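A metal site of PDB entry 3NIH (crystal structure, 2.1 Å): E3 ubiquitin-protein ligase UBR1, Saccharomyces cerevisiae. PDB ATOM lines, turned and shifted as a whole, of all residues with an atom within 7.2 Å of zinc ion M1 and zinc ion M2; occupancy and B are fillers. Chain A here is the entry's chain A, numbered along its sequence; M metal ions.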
ATOM      1  N   HIS A   4     -29.267  -1.042  33.905  1.00  0.00           N
ATOM      2  CA  HIS A   4     -28.640  -1.907  32.893  1.00  0.00           C
ATOM      3  C   HIS A   4     -27.111  -1.900  32.925  1.00  0.00           C
ATOM      4  O   HIS A   4     -26.470  -2.497  32.051  1.00  0.00           O
ATOM      5  CB  HIS A   4     -29.125  -1.506  31.510  1.00  0.00           C
ATOM      6  CG  HIS A   4     -30.563  -1.088  31.470  1.00  0.00           C
ATOM      7  ND1 HIS A   4     -31.603  -1.987  31.550  1.00  0.00           N
ATOM      8  CD2 HIS A   4     -31.125   0.134  31.355  1.00  0.00           C
ATOM      9  CE1 HIS A   4     -32.753  -1.329  31.484  1.00  0.00           C
ATOM     10  NE2 HIS A   4     -32.490  -0.045  31.356  1.00  0.00           N
ATOM     11  N   LYS A   5     -26.526  -1.239  33.928  1.00  0.00           N
ATOM     12  CA  LYS A   5     -25.093  -1.280  34.156  1.00  0.00           C
ATOM     13  C   LYS A   5     -24.654  -2.734  34.314  1.00  0.00           C
ATOM     14  O   LYS A   5     -25.355  -3.541  34.916  1.00  0.00           O
ATOM     15  CB  LYS A   5     -24.702  -0.507  35.422  1.00  0.00           C
ATOM     16  CG  LYS A   5     -24.611   0.997  35.279  1.00  0.00           C
ATOM     17  CD  LYS A   5     -25.725   1.707  36.032  1.00  0.00           C
ATOM     18  CE  LYS A   5     -25.356   3.159  36.319  1.00  0.00           C
ATOM     19  NZ  LYS A   5     -26.477   3.923  36.944  1.00  0.00           N
ATOM     20  N   HIS A   6     -23.490  -3.049  33.753  1.00  0.00           N
ATOM     21  CA  HIS A   6     -22.905  -4.378  33.912  1.00  0.00           C
ATOM     22  C   HIS A   6     -21.400  -4.202  34.084  1.00  0.00           C
ATOM     23  O   HIS A   6     -20.590  -4.960  33.522  1.00  0.00           O
ATOM     24  CB  HIS A   6     -23.246  -5.256  32.711  1.00  0.00           C
ATOM     25  CG  HIS A   6     -22.751  -4.707  31.405  1.00  0.00           C
ATOM     26  ND1 HIS A   6     -21.490  -4.994  30.924  1.00  0.00           N
ATOM     27  CD2 HIS A   6     -23.330  -3.897  30.499  1.00  0.00           C
ATOM     28  CE1 HIS A   6     -21.323  -4.378  29.770  1.00  0.00           C
ATOM     29  NE2 HIS A   6     -22.429  -3.714  29.482  1.00  0.00           N
ATOM     30  N   ARG A   9     -17.958  -6.595  33.458  1.00  0.00           N
ATOM     31  CA  ARG A   9     -18.282  -7.841  32.761  1.00  0.00           C
ATOM     32  C   ARG A   9     -19.028  -7.523  31.467  1.00  0.00           C
ATOM     33  O   ARG A   9     -19.329  -6.367  31.178  1.00  0.00           O
ATOM     34  CB  ARG A   9     -19.091  -8.799  33.649  1.00  0.00           C
ATOM     35  CG  ARG A   9     -20.307  -8.179  34.341  1.00  0.00           C
ATOM     36  CD  ARG A   9     -21.356  -9.228  34.697  1.00  0.00           C
ATOM     37  NE  ARG A   9     -22.206  -9.546  33.525  1.00  0.00           N
ATOM     38  CZ  ARG A   9     -23.345 -10.238  33.588  1.00  0.00           C
ATOM     39  NH1 ARG A   9     -23.792 -10.715  34.770  1.00  0.00           N
ATOM     40  NH2 ARG A   9     -24.043 -10.458  32.453  1.00  0.00           N
ATOM     41  N   ASN A  10     -19.290  -8.557  30.674  1.00  0.00           N
ATOM     42  CA  ASN A  10     -20.020  -8.381  29.430  1.00  0.00           C
ATOM     43  C   ASN A  10     -21.496  -8.091  29.744  1.00  0.00           C
ATOM     44  O   ASN A  10     -22.010  -8.471  30.806  1.00  0.00           O
ATOM     45  CB  ASN A  10     -19.917  -9.647  28.590  1.00  0.00           C
ATOM     46  CG  ASN A  10     -20.642 -10.822  29.214  1.00  0.00           C
ATOM     47  OD1 ASN A  10     -20.369 -11.201  30.361  1.00  0.00           O
ATOM     48  ND2 ASN A  10     -21.574 -11.398  28.476  1.00  0.00           N
ATOM     49  N   CYS A  11     -22.175  -7.429  28.811  1.00  0.00           N
ATOM     50  CA  CYS A  11     -23.603  -7.219  28.950  1.00  0.00           C
ATOM     51  C   CYS A  11     -24.330  -8.544  28.805  1.00  0.00           C
ATOM     52  O   CYS A  11     -24.928  -9.041  29.766  1.00  0.00           O
ATOM     53  CB  CYS A  11     -24.124  -6.197  27.925  1.00  0.00           C
ATOM     54  SG  CYS A  11     -25.910  -6.000  28.023  1.00  0.00           S
ATOM     55  N   GLY A  12     -24.271  -9.128  27.618  1.00  0.00           N
ATOM     56  CA  GLY A  12     -24.926 -10.407  27.358  1.00  0.00           C
ATOM     57  C   GLY A  12     -26.453 -10.350  27.354  1.00  0.00           C
ATOM     58  O   GLY A  12     -27.109 -11.387  27.342  1.00  0.00           O
ATOM     59  N   ARG A  13     -27.006  -9.136  27.387  1.00  0.00           N
ATOM     60  CA  ARG A  13     -28.473  -8.956  27.318  1.00  0.00           C
ATOM     61  C   ARG A  13     -29.022  -9.633  26.070  1.00  0.00           C
ATOM     62  O   ARG A  13     -28.600  -9.326  24.957  1.00  0.00           O
ATOM     63  CB  ARG A  13     -28.852  -7.475  27.296  1.00  0.00           C
ATOM     64  CG  ARG A  13     -30.350  -7.185  27.102  1.00  0.00           C
ATOM     65  CD  ARG A  13     -30.641  -5.696  27.181  1.00  0.00           C
ATOM     66  NE  ARG A  13     -30.982  -5.307  28.542  1.00  0.00           N
ATOM     67  CZ  ARG A  13     -32.224  -5.350  29.030  1.00  0.00           C
ATOM     68  NH1 ARG A  13     -33.227  -5.738  28.242  1.00  0.00           N
ATOM     69  NH2 ARG A  13     -32.465  -4.986  30.290  1.00  0.00           N
ATOM     70  N   PHE A  15     -31.532 -10.226  23.161  1.00  0.00           N
ATOM     71  CA  PHE A  15     -32.502  -9.457  22.385  1.00  0.00           C
ATOM     72  C   PHE A  15     -33.835 -10.195  22.291  1.00  0.00           C
ATOM     73  O   PHE A  15     -33.872 -11.420  22.182  1.00  0.00           O
ATOM     74  CB  PHE A  15     -31.984  -9.157  20.973  1.00  0.00           C
ATOM     75  CG  PHE A  15     -30.782  -8.256  20.951  1.00  0.00           C
ATOM     76  CD1 PHE A  15     -30.930  -6.876  21.093  1.00  0.00           C
ATOM     77  CD2 PHE A  15     -29.509  -8.785  20.807  1.00  0.00           C
ATOM     78  CE1 PHE A  15     -29.814  -6.042  21.082  1.00  0.00           C
ATOM     79  CE2 PHE A  15     -28.371  -7.950  20.792  1.00  0.00           C
ATOM     80  CZ  PHE A  15     -28.523  -6.592  20.935  1.00  0.00           C
ATOM     81  N   VAL A  34     -22.693  -6.832  18.139  1.00  0.00           N
ATOM     82  CA  VAL A  34     -23.867  -5.978  18.304  1.00  0.00           C
ATOM     83  C   VAL A  34     -23.970  -5.382  19.721  1.00  0.00           C
ATOM     84  O   VAL A  34     -23.427  -5.929  20.678  1.00  0.00           O
ATOM     85  CB  VAL A  34     -25.193  -6.750  17.983  1.00  0.00           C
ATOM     86  CG1 VAL A  34     -26.390  -5.813  17.981  1.00  0.00           C
ATOM     87  CG2 VAL A  34     -25.127  -7.450  16.636  1.00  0.00           C
ATOM     88  N   LEU A  35     -24.705  -4.275  19.816  1.00  0.00           N
ATOM     89  CA  LEU A  35     -24.966  -3.572  21.073  1.00  0.00           C
ATOM     90  C   LEU A  35     -26.460  -3.395  21.244  1.00  0.00           C
ATOM     91  O   LEU A  35     -27.174  -3.151  20.273  1.00  0.00           O
ATOM     92  CB  LEU A  35     -24.325  -2.189  21.040  1.00  0.00           C
ATOM     93  CG  LEU A  35     -22.785  -2.174  21.000  1.00  0.00           C
ATOM     94  CD1 LEU A  35     -22.276  -0.813  20.570  1.00  0.00           C
ATOM     95  CD2 LEU A  35     -22.260  -2.541  22.377  1.00  0.00           C
ATOM     96  N   CYS A  36     -26.941  -3.523  22.478  1.00  0.00           N
ATOM     97  CA  CYS A  36     -28.331  -3.194  22.771  1.00  0.00           C
ATOM     98  C   CYS A  36     -28.500  -1.683  22.915  1.00  0.00           C
ATOM     99  O   CYS A  36     -27.520  -0.941  22.954  1.00  0.00           O
ATOM    100  CB  CYS A  36     -28.838  -3.916  24.024  1.00  0.00           C
ATOM    101  SG  CYS A  36     -28.144  -3.358  25.616  1.00  0.00           S
ATOM    102  N   ILE A  37     -29.761  -1.253  23.034  1.00  0.00           N
ATOM    103  CA  ILE A  37     -30.101   0.173  23.139  1.00  0.00           C
ATOM    104  C   ILE A  37     -29.635   0.799  24.462  1.00  0.00           C
ATOM    105  O   ILE A  37     -29.359   1.990  24.528  1.00  0.00           O
ATOM    106  CB  ILE A  37     -31.627   0.409  22.867  1.00  0.00           C
ATOM    107  CG1 ILE A  37     -31.897   1.892  22.576  1.00  0.00           C
ATOM    108  CG2 ILE A  37     -32.486  -0.165  24.034  1.00  0.00           C
ATOM    109  CD1 ILE A  37     -33.249   2.182  21.911  1.00  0.00           C
ATOM    110  N   HIS A  38     -29.528  -0.010  25.508  1.00  0.00           N
ATOM    111  CA  HIS A  38     -29.057   0.474  26.808  1.00  0.00           C
ATOM    112  C   HIS A  38     -27.535   0.672  26.825  1.00  0.00           C
ATOM    113  O   HIS A  38     -27.014   1.396  27.684  1.00  0.00           O
ATOM    114  CB  HIS A  38     -29.487  -0.476  27.926  1.00  0.00           C
ATOM    115  CG  HIS A  38     -30.947  -0.756  27.942  1.00  0.00           C
ATOM    116  ND1 HIS A  38     -31.464  -2.035  27.823  1.00  0.00           N
ATOM    117  CD2 HIS A  38     -32.014   0.070  28.009  1.00  0.00           C
ATOM    118  CE1 HIS A  38     -32.778  -1.976  27.849  1.00  0.00           C
ATOM    119  NE2 HIS A  38     -33.145  -0.714  27.956  1.00  0.00           N
ATOM    120  N   CYS A  39     -26.843   0.032  25.895  1.00  0.00           N
ATOM    121  CA  CYS A  39     -25.382  -0.015  25.880  1.00  0.00           C
ATOM    122  C   CYS A  39     -24.799   0.929  24.814  1.00  0.00           C
ATOM    123  O   CYS A  39     -23.779   1.590  25.038  1.00  0.00           O
ATOM    124  CB  CYS A  39     -24.900  -1.465  25.667  1.00  0.00           C
ATOM    125  SG  CYS A  39     -25.136  -2.663  27.069  1.00  0.00           S
ATOM    126  N   PHE A  40     -25.455   0.992  23.652  1.00  0.00           N
ATOM    127  CA  PHE A  40     -25.002   1.829  22.541  1.00  0.00           C
ATOM    128  C   PHE A  40     -24.927   3.308  22.918  1.00  0.00           C
ATOM    129  O   PHE A  40     -25.920   3.924  23.344  1.00  0.00           O
ATOM    130  CB  PHE A  40     -25.888   1.628  21.303  1.00  0.00           C
ATOM    131  CG  PHE A  40     -25.501   2.510  20.119  1.00  0.00           C
ATOM    132  CD1 PHE A  40     -24.527   2.099  19.213  1.00  0.00           C
ATOM    133  CD2 PHE A  40     -26.135   3.727  19.920  1.00  0.00           C
ATOM    134  CE1 PHE A  40     -24.188   2.912  18.120  1.00  0.00           C
ATOM    135  CE2 PHE A  40     -25.795   4.558  18.835  1.00  0.00           C
ATOM    136  CZ  PHE A  40     -24.814   4.142  17.940  1.00  0.00           C
ATOM    137  N   ILE A  62     -27.211 -11.915  21.624  1.00  0.00           N
ATOM    138  CA  ILE A  62     -26.848 -11.198  22.845  1.00  0.00           C
ATOM    139  C   ILE A  62     -25.961  -9.996  22.552  1.00  0.00           C
ATOM    140  O   ILE A  62     -25.200  -9.986  21.595  1.00  0.00           O
ATOM    141  CB  ILE A  62     -26.134 -12.112  23.881  1.00  0.00           C
ATOM    142  CG1 ILE A  62     -24.858 -12.710  23.288  1.00  0.00           C
ATOM    143  CG2 ILE A  62     -27.096 -13.215  24.383  1.00  0.00           C
ATOM    144  CD1 ILE A  62     -23.828 -13.184  24.311  1.00  0.00           C
ATOM    145  N   CYS A  63     -26.072  -8.990  23.418  1.00  0.00           N
ATOM    146  CA  CYS A  63     -25.323  -7.757  23.293  1.00  0.00           C
ATOM    147  C   CYS A  63     -23.865  -8.027  23.674  1.00  0.00           C
ATOM    148  O   CYS A  63     -23.608  -8.729  24.659  1.00  0.00           O
ATOM    149  CB  CYS A  63     -25.922  -6.698  24.202  1.00  0.00           C
ATOM    150  SG  CYS A  63     -24.868  -5.298  24.424  1.00  0.00           S
ATOM    151  N   ASP A  64     -22.941  -7.494  22.878  1.00  0.00           N
ATOM    152  CA  ASP A  64     -21.499  -7.753  23.030  1.00  0.00           C
ATOM    153  C   ASP A  64     -20.742  -6.668  23.815  1.00  0.00           C
ATOM    154  O   ASP A  64     -19.517  -6.736  23.947  1.00  0.00           O
ATOM    155  CB  ASP A  64     -20.829  -7.981  21.671  1.00  0.00           C
ATOM    156  CG  ASP A  64     -21.405  -9.167  20.931  1.00  0.00           C
ATOM    157  OD1 ASP A  64     -21.311 -10.301  21.440  1.00  0.00           O
ATOM    158  OD2 ASP A  64     -21.973  -8.972  19.832  1.00  0.00           O
ATOM    159  N   CYS A  65     -21.483  -5.688  24.334  1.00  0.00           N
ATOM    160  CA  CYS A  65     -20.868  -4.636  25.157  1.00  0.00           C
ATOM    161  C   CYS A  65     -20.088  -5.228  26.326  1.00  0.00           C
ATOM    162  O   CYS A  65     -20.605  -6.070  27.070  1.00  0.00           O
ATOM    163  CB  CYS A  65     -21.922  -3.683  25.690  1.00  0.00           C
ATOM    164  SG  CYS A  65     -21.208  -2.202  26.441  1.00  0.00           S
ATOM    165  N   GLY A  66     -18.839  -4.782  26.474  1.00  0.00           N
ATOM    166  CA  GLY A  66     -17.955  -5.298  27.507  1.00  0.00           C
ATOM    167  C   GLY A  66     -17.214  -6.573  27.117  1.00  0.00           C
ATOM    168  O   GLY A  66     -16.385  -7.069  27.877  1.00  0.00           O
ATOM    169  N   HIS A  76     -17.789   2.832  25.541  1.00  0.00           N
ATOM    170  CA  HIS A  76     -18.170   3.411  26.818  1.00  0.00           C
ATOM    171  C   HIS A  76     -19.680   3.265  27.009  1.00  0.00           C
ATOM    172  O   HIS A  76     -20.445   4.126  26.560  1.00  0.00           O
ATOM    173  CB  HIS A  76     -17.768   4.885  26.898  1.00  0.00           C
ATOM    174  CG  HIS A  76     -16.318   5.132  26.602  1.00  0.00           C
ATOM    175  ND1 HIS A  76     -15.844   5.350  25.335  1.00  0.00           N
ATOM    176  CD2 HIS A  76     -15.241   5.187  27.427  1.00  0.00           C
ATOM    177  CE1 HIS A  76     -14.541   5.537  25.372  1.00  0.00           C
ATOM    178  NE2 HIS A  76     -14.150   5.452  26.636  1.00  0.00           N
ATOM    179  N   CYS A  77     -20.078   2.177  27.682  1.00  0.00           N
ATOM    180  CA  CYS A  77     -21.477   1.804  27.910  1.00  0.00           C
ATOM    181  C   CYS A  77     -22.338   3.033  28.216  1.00  0.00           C
ATOM    182  O   CYS A  77     -22.024   3.808  29.126  1.00  0.00           O
ATOM    183  CB  CYS A  77     -21.564   0.779  29.072  1.00  0.00           C
ATOM    184  SG  CYS A  77     -22.939  -0.436  29.006  1.00  0.00           S
ATOM    185  N   LYS A  78     -23.417   3.203  27.449  1.00  0.00           N
ATOM    186  CA  LYS A  78     -24.390   4.272  27.729  1.00  0.00           C
ATOM    187  C   LYS A  78     -24.985   4.140  29.137  1.00  0.00           C
ATOM    188  O   LYS A  78     -25.162   5.135  29.828  1.00  0.00           O
ATOM    189  CB  LYS A  78     -25.515   4.312  26.687  1.00  0.00           C
ATOM    190  CG  LYS A  78     -26.386   5.586  26.758  1.00  0.00           C
ATOM    191  CD  LYS A  78     -27.620   5.487  25.871  1.00  0.00           C
ATOM    192  CE  LYS A  78     -28.396   6.799  25.820  1.00  0.00           C
ATOM    193  NZ  LYS A  78     -29.234   7.040  27.035  1.00  0.00           N
ATOM    194  N   ALA A  79     -25.269   2.898  29.548  1.00  0.00           N
ATOM    195  CA  ALA A  79     -25.826   2.611  30.883  1.00  0.00           C
ATOM    196  C   ALA A  79     -24.903   3.060  32.021  1.00  0.00           C
ATOM    197  O   ALA A  79     -25.368   3.323  33.127  1.00  0.00           O
ATOM    198  CB  ALA A  79     -26.154   1.129  31.020  1.00  0.00           C
ATOM    199  N   GLU A  80     -23.601   3.169  31.730  1.00  0.00           N
ATOM    200  CA  GLU A  80     -22.597   3.575  32.708  1.00  0.00           C
ATOM    201  C   GLU A  80     -22.556   5.102  32.898  1.00  0.00           C
ATOM    202  O   GLU A  80     -21.833   5.606  33.772  1.00  0.00           O
ATOM    203  CB  GLU A  80     -21.215   3.047  32.296  1.00  0.00           C
ATOM    204  CG  GLU A  80     -20.270   2.721  33.440  1.00  0.00           C
ATOM    205  CD  GLU A  80     -20.779   1.598  34.333  1.00  0.00           C
ATOM    206  OE1 GLU A  80     -21.001   0.474  33.824  1.00  0.00           O
ATOM    207  OE2 GLU A  80     -20.943   1.837  35.546  1.00  0.00           O
HETATM  208 ZN    ZN M   1     -26.087  -4.350  26.184  1.00  0.00          ZN
HETATM  209 ZN    ZN M   2     -23.124  -2.055  28.021  1.00  0.00          ZN
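The backbone carbonyl oxygen (O) of Cys 39 lies within hydrogen-bond range of the backbone NH (N) of Lys 78.
ND1 of His 6 sits at hydrogen-bond distance from N of Cys 11.
ND1 of His 6 is in hydrogen-bond range of O of Arg 9 (2.6 Å).
The side-chain sulfur (SG) of Cys 63 sits close to the backbone NH (N) of Cys 65 (3.4 Å).
The backbone NH of Cys 63 is in hydrogen-bond range of the backbone carbonyl oxygen of Arg 13, 3.0 Å away.
The backbone carbonyl oxygen (O) of Cys 63 is in hydrogen-bond range of the backbone NH (N) of Gly 12 (3.1 Å).
SG of Cys 36 sits close to N of His 38.
The guanidinium group of Arg 9 lies within hydrogen-bond range of the backbone carbonyl oxygen of Cys 11, 3.2 Å away.
The nearest printed residue that does not touch zinc ion M1 is Cys 65 (4.2 Å).
Zinc ion M1 is bound by the side-chain sulfur (SG) of Cys 39 (2.1 Å).
The side-chain sulfur (SG) of Cys 63 is bound to zinc ion M1.
Zinc ion M1 is bound by the side-chain sulfur (SG) of Cys 36, 2.4 Å away.
SG of Cys 11 is bound to zinc ion M1 (2.5 Å).
Four residues have an atom within 4 Å of zinc ion M2: His 6, Cys 39, Cys 65 and Cys 77.
The nearest printed residue that does not touch zinc ion M2 is Cys 11 (4.3 Å).
Zinc ion M2 is bound by the side-chain sulfur of Cys 77, the side-chain sulfur of Cys 39, a ring nitrogen (NE2) of His 6 and the side-chain sulfur of Cys 65.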
